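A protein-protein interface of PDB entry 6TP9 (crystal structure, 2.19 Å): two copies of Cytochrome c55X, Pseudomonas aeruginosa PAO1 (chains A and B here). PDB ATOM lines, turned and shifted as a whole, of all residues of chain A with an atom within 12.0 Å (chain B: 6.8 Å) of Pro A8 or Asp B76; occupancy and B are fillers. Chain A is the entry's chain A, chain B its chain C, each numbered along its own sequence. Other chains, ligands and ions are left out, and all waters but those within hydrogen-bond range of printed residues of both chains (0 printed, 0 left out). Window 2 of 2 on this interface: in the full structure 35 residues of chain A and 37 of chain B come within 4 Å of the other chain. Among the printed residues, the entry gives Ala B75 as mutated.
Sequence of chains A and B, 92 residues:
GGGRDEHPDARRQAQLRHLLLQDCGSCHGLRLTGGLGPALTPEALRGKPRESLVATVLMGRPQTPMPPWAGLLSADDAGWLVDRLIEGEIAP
NH2 of Arg A12 is in salt-bridge range of OD2 of Asp B77, at 2.6 Å.
OE1 of Gln A13 is in hydrogen-bond range of NE1 of Trp B80 (3.5 Å).
The backbone carbonyl oxygen (O) of Pro A8 is in hydrogen-bond range of the side-chain amide nitrogen (NE2) of Gln A13 (3.1 Å).
The side-chain carboxylate (OD1) of Asp A9 lies within hydrogen-bond range of the backbone NH (N) of Arg A12 (2.9 Å).
The backbone NH of Asp B76 sits close to the side-chain hydroxyl of Ser B74, at 3.4 Å.
N of Ser B74 lies within hydrogen-bond range of OD2 of Asp B77 (3.0 Å).
Among the printed residues, pairs that only touch across the chains: Pro A8 with Asp B76, Pro A8 with Asp B77, Pro A8 with Trp B80, Arg A12 with Leu B73, Leu A16 with Leu B73, Leu A16 with Asp B77, Leu A16 with Trp B80, Leu A16 with Leu B81 and Arg A17 with Trp B80.
Printed residues of chain B within 4 Å of Pro A8: Asp B76, Asp B77 and Trp B80.
No residue of chain A comes within 4 Å of Ser B74.
No residue of chain A comes within 4 Å of Ala B75.
Asp B77 touches three residues of chain A.
No residue of chain A comes within 4 Å of Ala B78.
No residue of chain A comes within 4 Å of Gly B79.
Of the printed residues of chain A, Leu B81 touches Leu A16 (3.5 Å).
Of the printed residues of chain B, Gln A13 touches Trp B80 (3.5 Å).
Of the printed residues of chain A, Leu B73 touches Arg A12 and Leu A16.
Ala A10 touches none of the printed residues of chain B.
Arg B50 touches none of the printed residues of chain A.
The nearest printed residue of chain A that does not touch Asp B76 is Leu A16 (5.8 Å).
Of the 13 printed residues of chain A, 5 touch a printed residue of chain B.
Hydrophobic or aromatic side chains of chain A that line the printed part of chain B: Pro A8 and Leu A16.
Hydrophobic or aromatic side chains of chain B within 4 Å of the printed part of chain A: Leu B73, Trp B80 and Leu B81.
Among the printed residues, 11 pairs touch across the chains.
Among the printed residues, Asp or Glu carboxylates within 4 Å of a Lys or Arg side-chain nitrogen of the other chain: Arg A12 with Asp B77 (2.6 Å).
No position is printed for both chains.
Of the 11 pairs that touch across the chains among the printed residues, none has its exchanged pair printed and touching as well.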
ATOM      1  N   PRO A   8     -16.621 -14.733  10.461  1.00  0.00           N
ATOM      2  CA  PRO A   8     -17.854 -14.357  11.165  1.00  0.00           C
ATOM      3  C   PRO A   8     -18.509 -13.121  10.561  1.00  0.00           C
ATOM      4  O   PRO A   8     -17.810 -12.161  10.241  1.00  0.00           O
ATOM      5  CB  PRO A   8     -17.376 -14.073  12.596  1.00  0.00           C
ATOM      6  CG  PRO A   8     -16.045 -14.742  12.710  1.00  0.00           C
ATOM      7  CD  PRO A   8     -15.444 -14.674  11.342  1.00  0.00           C
ATOM      8  N   ASP A   9     -19.831 -13.137  10.420  1.00  0.00           N
ATOM      9  CA  ASP A   9     -20.536 -12.033   9.791  1.00  0.00           C
ATOM     10  C   ASP A   9     -20.845 -10.941  10.816  1.00  0.00           C
ATOM     11  O   ASP A   9     -20.504 -11.039  11.997  1.00  0.00           O
ATOM     12  CB  ASP A   9     -21.810 -12.534   9.106  1.00  0.00           C
ATOM     13  CG  ASP A   9     -22.840 -13.078  10.085  1.00  0.00           C
ATOM     14  OD1 ASP A   9     -22.734 -12.808  11.299  1.00  0.00           O
ATOM     15  OD2 ASP A   9     -23.764 -13.788   9.634  1.00  0.00           O
ATOM     16  N   ALA A  10     -21.520  -9.890  10.348  1.00  0.00           N
ATOM     17  CA  ALA A  10     -21.803  -8.725  11.180  1.00  0.00           C
ATOM     18  C   ALA A  10     -22.405  -9.121  12.525  1.00  0.00           C
ATOM     19  O   ALA A  10     -21.821  -8.862  13.583  1.00  0.00           O
ATOM     20  CB  ALA A  10     -22.747  -7.782  10.429  1.00  0.00           C
ATOM     21  N   ARG A  11     -23.587  -9.740  12.499  1.00  0.00           N
ATOM     22  CA  ARG A  11     -24.281 -10.056  13.744  1.00  0.00           C
ATOM     23  C   ARG A  11     -23.427 -10.936  14.646  1.00  0.00           C
ATOM     24  O   ARG A  11     -23.463 -10.800  15.875  1.00  0.00           O
ATOM     25  CB  ARG A  11     -25.617 -10.738  13.441  1.00  0.00           C
ATOM     26  N   ARG A  12     -22.647 -11.843  14.053  1.00  0.00           N
ATOM     27  CA  ARG A  12     -21.834 -12.757  14.850  1.00  0.00           C
ATOM     28  C   ARG A  12     -20.683 -12.026  15.529  1.00  0.00           C
ATOM     29  O   ARG A  12     -20.403 -12.264  16.710  1.00  0.00           O
ATOM     30  CB  ARG A  12     -21.310 -13.885  13.963  1.00  0.00           C
ATOM     31  CG  ARG A  12     -20.446 -14.911  14.678  1.00  0.00           C
ATOM     32  CD  ARG A  12     -21.190 -15.613  15.802  1.00  0.00           C
ATOM     33  NE  ARG A  12     -20.485 -16.821  16.227  1.00  0.00           N
ATOM     34  CZ  ARG A  12     -20.706 -17.466  17.368  1.00  0.00           C
ATOM     35  NH1 ARG A  12     -21.616 -17.022  18.224  1.00  0.00           N
ATOM     36  NH2 ARG A  12     -20.010 -18.555  17.654  1.00  0.00           N
ATOM     37  N   GLN A  13     -20.003 -11.135  14.804  1.00  0.00           N
ATOM     38  CA  GLN A  13     -18.916 -10.374  15.409  1.00  0.00           C
ATOM     39  C   GLN A  13     -19.387  -9.657  16.668  1.00  0.00           C
ATOM     40  O   GLN A  13     -18.635  -9.530  17.640  1.00  0.00           O
ATOM     41  CB  GLN A  13     -18.347  -9.371  14.404  1.00  0.00           C
ATOM     42  CG  GLN A  13     -17.699 -10.008  13.185  1.00  0.00           C
ATOM     43  CD  GLN A  13     -17.029  -8.989  12.284  1.00  0.00           C
ATOM     44  OE1 GLN A  13     -16.527  -7.966  12.750  1.00  0.00           O
ATOM     45  NE2 GLN A  13     -17.024  -9.261  10.983  1.00  0.00           N
ATOM     46  N   ALA A  14     -20.637  -9.188  16.672  1.00  0.00           N
ATOM     47  CA  ALA A  14     -21.167  -8.517  17.853  1.00  0.00           C
ATOM     48  C   ALA A  14     -21.332  -9.491  19.014  1.00  0.00           C
ATOM     49  O   ALA A  14     -20.995  -9.165  20.158  1.00  0.00           O
ATOM     50  CB  ALA A  14     -22.500  -7.847  17.520  1.00  0.00           C
ATOM     51  N   GLN A  15     -21.856 -10.688  18.740  1.00  0.00           N
ATOM     52  CA  GLN A  15     -21.961 -11.699  19.787  1.00  0.00           C
ATOM     53  C   GLN A  15     -20.600 -12.002  20.393  1.00  0.00           C
ATOM     54  O   GLN A  15     -20.469 -12.148  21.613  1.00  0.00           O
ATOM     55  CB  GLN A  15     -22.566 -12.981  19.226  1.00  0.00           C
ATOM     56  CG  GLN A  15     -24.062 -12.971  19.081  1.00  0.00           C
ATOM     57  CD  GLN A  15     -24.586 -14.305  18.599  1.00  0.00           C
ATOM     58  OE1 GLN A  15     -25.074 -15.116  19.386  1.00  0.00           O
ATOM     59  NE2 GLN A  15     -24.473 -14.547  17.298  1.00  0.00           N
ATOM     60  N   LEU A  16     -19.578 -12.123  19.547  1.00  0.00           N
ATOM     61  CA  LEU A  16     -18.243 -12.432  20.038  1.00  0.00           C
ATOM     62  C   LEU A  16     -17.681 -11.277  20.857  1.00  0.00           C
ATOM     63  O   LEU A  16     -17.037 -11.499  21.890  1.00  0.00           O
ATOM     64  CB  LEU A  16     -17.332 -12.769  18.857  1.00  0.00           C
ATOM     65  CG  LEU A  16     -17.875 -13.891  17.966  1.00  0.00           C
ATOM     66  CD1 LEU A  16     -17.040 -14.048  16.707  1.00  0.00           C
ATOM     67  CD2 LEU A  16     -17.944 -15.207  18.727  1.00  0.00           C
ATOM     68  N   ARG A  17     -17.923 -10.037  20.423  1.00  0.00           N
ATOM     69  CA  ARG A  17     -17.503  -8.887  21.218  1.00  0.00           C
ATOM     70  C   ARG A  17     -18.192  -8.879  22.574  1.00  0.00           C
ATOM     71  O   ARG A  17     -17.557  -8.613  23.601  1.00  0.00           O
ATOM     72  CB  ARG A  17     -17.792  -7.587  20.469  1.00  0.00           C
ATOM     73  CG  ARG A  17     -16.909  -7.364  19.259  1.00  0.00           C
ATOM     74  CD  ARG A  17     -17.105  -5.982  18.659  1.00  0.00           C
ATOM     75  NE  ARG A  17     -16.156  -5.708  17.582  1.00  0.00           N
ATOM     76  CZ  ARG A  17     -14.896  -5.326  17.770  1.00  0.00           C
ATOM     77  NH1 ARG A  17     -14.417  -5.178  18.999  1.00  0.00           N
ATOM     78  NH2 ARG A  17     -14.110  -5.096  16.728  1.00  0.00           N
ATOM     79  N   HIS A  18     -19.495  -9.162  22.602  1.00  0.00           N
ATOM     80  CA  HIS A  18     -20.201  -9.217  23.877  1.00  0.00           C
ATOM     81  C   HIS A  18     -19.646 -10.332  24.752  1.00  0.00           C
ATOM     82  O   HIS A  18     -19.334 -10.120  25.930  1.00  0.00           O
ATOM     83  CB  HIS A  18     -21.698  -9.410  23.644  1.00  0.00           C
ATOM     84  CG  HIS A  18     -22.520  -9.234  24.880  1.00  0.00           C
ATOM     85  ND1 HIS A  18     -23.476 -10.146  25.276  1.00  0.00           N
ATOM     86  CD2 HIS A  18     -22.519  -8.258  25.818  1.00  0.00           C
ATOM     87  CE1 HIS A  18     -24.033  -9.736  26.401  1.00  0.00           C
ATOM     88  NE2 HIS A  18     -23.469  -8.593  26.752  1.00  0.00           N
ATOM     89  N   LEU A  19     -19.509 -11.532  24.185  1.00  0.00           N
ATOM     90  CA  LEU A  19     -18.947 -12.654  24.928  1.00  0.00           C
ATOM     91  C   LEU A  19     -17.588 -12.292  25.516  1.00  0.00           C
ATOM     92  O   LEU A  19     -17.314 -12.552  26.693  1.00  0.00           O
ATOM     93  CB  LEU A  19     -18.828 -13.874  24.014  1.00  0.00           C
ATOM     94  CG  LEU A  19     -18.208 -15.125  24.635  1.00  0.00           C
ATOM     95  CD1 LEU A  19     -19.176 -15.773  25.612  1.00  0.00           C
ATOM     96  CD2 LEU A  19     -17.790 -16.102  23.551  1.00  0.00           C
ATOM     97  N   LEU A  20     -16.722 -11.687  24.700  1.00  0.00           N
ATOM     98  CA  LEU A  20     -15.390 -11.328  25.175  1.00  0.00           C
ATOM     99  C   LEU A  20     -15.466 -10.391  26.372  1.00  0.00           C
ATOM    100  O   LEU A  20     -14.749 -10.571  27.365  1.00  0.00           O
ATOM    101  CB  LEU A  20     -14.593 -10.676  24.043  1.00  0.00           C
ATOM    102  CG  LEU A  20     -13.165 -10.246  24.388  1.00  0.00           C
ATOM    103  CD1 LEU A  20     -12.303 -11.449  24.722  1.00  0.00           C
ATOM    104  CD2 LEU A  20     -12.556  -9.456  23.238  1.00  0.00           C
ATOM    105  N   ARG B  50      -0.111 -17.370  16.997  1.00  0.00           N
ATOM    106  CA  ARG B  50      -1.540 -17.081  16.961  1.00  0.00           C
ATOM    107  C   ARG B  50      -2.360 -18.361  17.070  1.00  0.00           C
ATOM    108  O   ARG B  50      -3.340 -18.422  17.819  1.00  0.00           O
ATOM    109  CB  ARG B  50      -1.894 -16.320  15.685  1.00  0.00           C
ATOM    110  CG  ARG B  50      -3.390 -16.210  15.418  1.00  0.00           C
ATOM    111  CD  ARG B  50      -3.668 -15.552  14.084  1.00  0.00           C
ATOM    112  NE  ARG B  50      -4.588 -16.353  13.283  1.00  0.00           N
ATOM    113  CZ  ARG B  50      -5.908 -16.192  13.257  1.00  0.00           C
ATOM    114  NH1 ARG B  50      -6.488 -15.247  13.984  1.00  0.00           N
ATOM    115  NH2 ARG B  50      -6.653 -16.981  12.494  1.00  0.00           N
ATOM    116  N   VAL B  54      -5.564 -19.608  19.590  1.00  0.00           N
ATOM    117  CA  VAL B  54      -6.832 -20.157  19.125  1.00  0.00           C
ATOM    118  C   VAL B  54      -7.038 -21.559  19.680  1.00  0.00           C
ATOM    119  O   VAL B  54      -8.158 -21.941  20.040  1.00  0.00           O
ATOM    120  CB  VAL B  54      -6.886 -20.142  17.588  1.00  0.00           C
ATOM    121  CG1 VAL B  54      -8.074 -20.951  17.091  1.00  0.00           C
ATOM    122  CG2 VAL B  54      -6.954 -18.711  17.082  1.00  0.00           C
ATOM    123  N   LEU B  58     -10.339 -22.944  21.908  1.00  0.00           N
ATOM    124  CA  LEU B  58     -11.244 -23.989  21.442  1.00  0.00           C
ATOM    125  C   LEU B  58     -11.258 -25.187  22.384  1.00  0.00           C
ATOM    126  O   LEU B  58     -12.305 -25.817  22.576  1.00  0.00           O
ATOM    127  CB  LEU B  58     -10.848 -24.432  20.034  1.00  0.00           C
ATOM    128  CG  LEU B  58     -11.026 -23.396  18.922  1.00  0.00           C
ATOM    129  CD1 LEU B  58     -10.477 -23.941  17.614  1.00  0.00           C
ATOM    130  CD2 LEU B  58     -12.486 -22.997  18.770  1.00  0.00           C
ATOM    131  N   LEU B  73     -17.918 -22.036  19.819  1.00  0.00           N
ATOM    132  CA  LEU B  73     -17.151 -21.231  18.884  1.00  0.00           C
ATOM    133  C   LEU B  73     -16.502 -22.121  17.837  1.00  0.00           C
ATOM    134  O   LEU B  73     -15.850 -23.114  18.174  1.00  0.00           O
ATOM    135  CB  LEU B  73     -16.078 -20.428  19.620  1.00  0.00           C
ATOM    136  CG  LEU B  73     -16.574 -19.548  20.765  1.00  0.00           C
ATOM    137  CD1 LEU B  73     -15.394 -18.833  21.397  1.00  0.00           C
ATOM    138  CD2 LEU B  73     -17.615 -18.553  20.284  1.00  0.00           C
ATOM    139  N   SER B  74     -16.681 -21.759  16.570  1.00  0.00           N
ATOM    140  CA  SER B  74     -15.955 -22.409  15.496  1.00  0.00           C
ATOM    141  C   SER B  74     -14.497 -21.952  15.509  1.00  0.00           C
ATOM    142  O   SER B  74     -14.085 -21.104  16.306  1.00  0.00           O
ATOM    143  CB  SER B  74     -16.604 -22.091  14.152  1.00  0.00           C
ATOM    144  OG  SER B  74     -16.490 -20.709  13.863  1.00  0.00           O
ATOM    145  N   ALA B  75     -13.703 -22.527  14.605  1.00  0.00           N
ATOM    146  CA  ALA B  75     -12.322 -22.085  14.457  1.00  0.00           C
ATOM    147  C   ALA B  75     -12.252 -20.675  13.885  1.00  0.00           C
ATOM    148  O   ALA B  75     -11.297 -19.940  14.160  1.00  0.00           O
ATOM    149  CB  ALA B  75     -11.553 -23.063  13.571  1.00  0.00           C
ATOM    150  N   ASP B  76     -13.249 -20.283  13.088  1.00  0.00           N
ATOM    151  CA  ASP B  76     -13.321 -18.907  12.610  1.00  0.00           C
ATOM    152  C   ASP B  76     -13.588 -17.950  13.763  1.00  0.00           C
ATOM    153  O   ASP B  76     -12.917 -16.920  13.901  1.00  0.00           O
ATOM    154  CB  ASP B  76     -14.413 -18.780  11.548  1.00  0.00           C
ATOM    155  CG  ASP B  76     -14.238 -19.764  10.410  1.00  0.00           C
ATOM    156  OD1 ASP B  76     -13.086 -19.963   9.967  1.00  0.00           O
ATOM    157  OD2 ASP B  76     -15.256 -20.339   9.962  1.00  0.00           O
ATOM    158  N   ASP B  77     -14.568 -18.279  14.606  1.00  0.00           N
ATOM    159  CA  ASP B  77     -14.893 -17.428  15.745  1.00  0.00           C
ATOM    160  C   ASP B  77     -13.679 -17.225  16.643  1.00  0.00           C
ATOM    161  O   ASP B  77     -13.334 -16.090  16.995  1.00  0.00           O
ATOM    162  CB  ASP B  77     -16.048 -18.043  16.535  1.00  0.00           C
ATOM    163  CG  ASP B  77     -17.292 -18.239  15.692  1.00  0.00           C
ATOM    164  OD1 ASP B  77     -17.498 -17.456  14.740  1.00  0.00           O
ATOM    165  OD2 ASP B  77     -18.063 -19.177  15.981  1.00  0.00           O
ATOM    166  N   ALA B  78     -13.017 -18.319  17.027  1.00  0.00           N
ATOM    167  CA  ALA B  78     -11.882 -18.209  17.938  1.00  0.00           C
ATOM    168  C   ALA B  78     -10.753 -17.399  17.315  1.00  0.00           C
ATOM    169  O   ALA B  78     -10.078 -16.626  18.006  1.00  0.00           O
ATOM    170  CB  ALA B  78     -11.387 -19.599  18.333  1.00  0.00           C
ATOM    171  N   GLY B  79     -10.530 -17.563  16.011  1.00  0.00           N
ATOM    172  CA  GLY B  79      -9.502 -16.779  15.348  1.00  0.00           C
ATOM    173  C   GLY B  79      -9.843 -15.304  15.308  1.00  0.00           C
ATOM    174  O   GLY B  79      -8.974 -14.449  15.502  1.00  0.00           O
ATOM    175  N   TRP B  80     -11.114 -14.982  15.063  1.00  0.00           N
ATOM    176  CA  TRP B  80     -11.535 -13.587  15.069  1.00  0.00           C
ATOM    177  C   TRP B  80     -11.266 -12.944  16.425  1.00  0.00           C
ATOM    178  O   TRP B  80     -10.616 -11.897  16.511  1.00  0.00           O
ATOM    179  CB  TRP B  80     -13.014 -13.489  14.702  1.00  0.00           C
ATOM    180  CG  TRP B  80     -13.479 -12.086  14.551  1.00  0.00           C
ATOM    181  CD1 TRP B  80     -13.414 -11.318  13.427  1.00  0.00           C
ATOM    182  CD2 TRP B  80     -14.076 -11.270  15.563  1.00  0.00           C
ATOM    183  NE1 TRP B  80     -13.938 -10.073  13.676  1.00  0.00           N
ATOM    184  CE2 TRP B  80     -14.352 -10.019  14.980  1.00  0.00           C
ATOM    185  CE3 TRP B  80     -14.406 -11.478  16.905  1.00  0.00           C
ATOM    186  CZ2 TRP B  80     -14.939  -8.980  15.691  1.00  0.00           C
ATOM    187  CZ3 TRP B  80     -14.991 -10.446  17.609  1.00  0.00           C
ATOM    188  CH2 TRP B  80     -15.251  -9.212  17.001  1.00  0.00           C
ATOM    189  N   LEU B  81     -11.757 -13.566  17.501  1.00  0.00           N
ATOM    190  CA  LEU B  81     -11.482 -13.057  18.840  1.00  0.00           C
ATOM    191  C   LEU B  81      -9.988 -12.854  19.054  1.00  0.00           C
ATOM    192  O   LEU B  81      -9.549 -11.787  19.497  1.00  0.00           O
ATOM    193  CB  LEU B  81     -12.039 -14.017  19.893  1.00  0.00           C
ATOM    194  CG  LEU B  81     -13.553 -14.047  20.103  1.00  0.00           C
ATOM    195  CD1 LEU B  81     -13.922 -15.172  21.059  1.00  0.00           C
ATOM    196  CD2 LEU B  81     -14.053 -12.711  20.631  1.00  0.00           C
ATOM    197  N   ASP B  83      -7.639 -12.376  16.973  1.00  0.00           N
ATOM    198  CA  ASP B  83      -7.190 -11.204  16.232  1.00  0.00           C
ATOM    199  C   ASP B  83      -7.533  -9.924  16.986  1.00  0.00           C
ATOM    200  O   ASP B  83      -6.701  -9.015  17.093  1.00  0.00           O
ATOM    201  CB  ASP B  83      -7.811 -11.198  14.836  1.00  0.00           C
ATOM    202  CG  ASP B  83      -7.234 -12.278  13.940  1.00  0.00           C
ATOM    203  OD1 ASP B  83      -6.095 -12.722  14.201  1.00  0.00           O
ATOM    204  OD2 ASP B  83      -7.916 -12.682  12.974  1.00  0.00           O
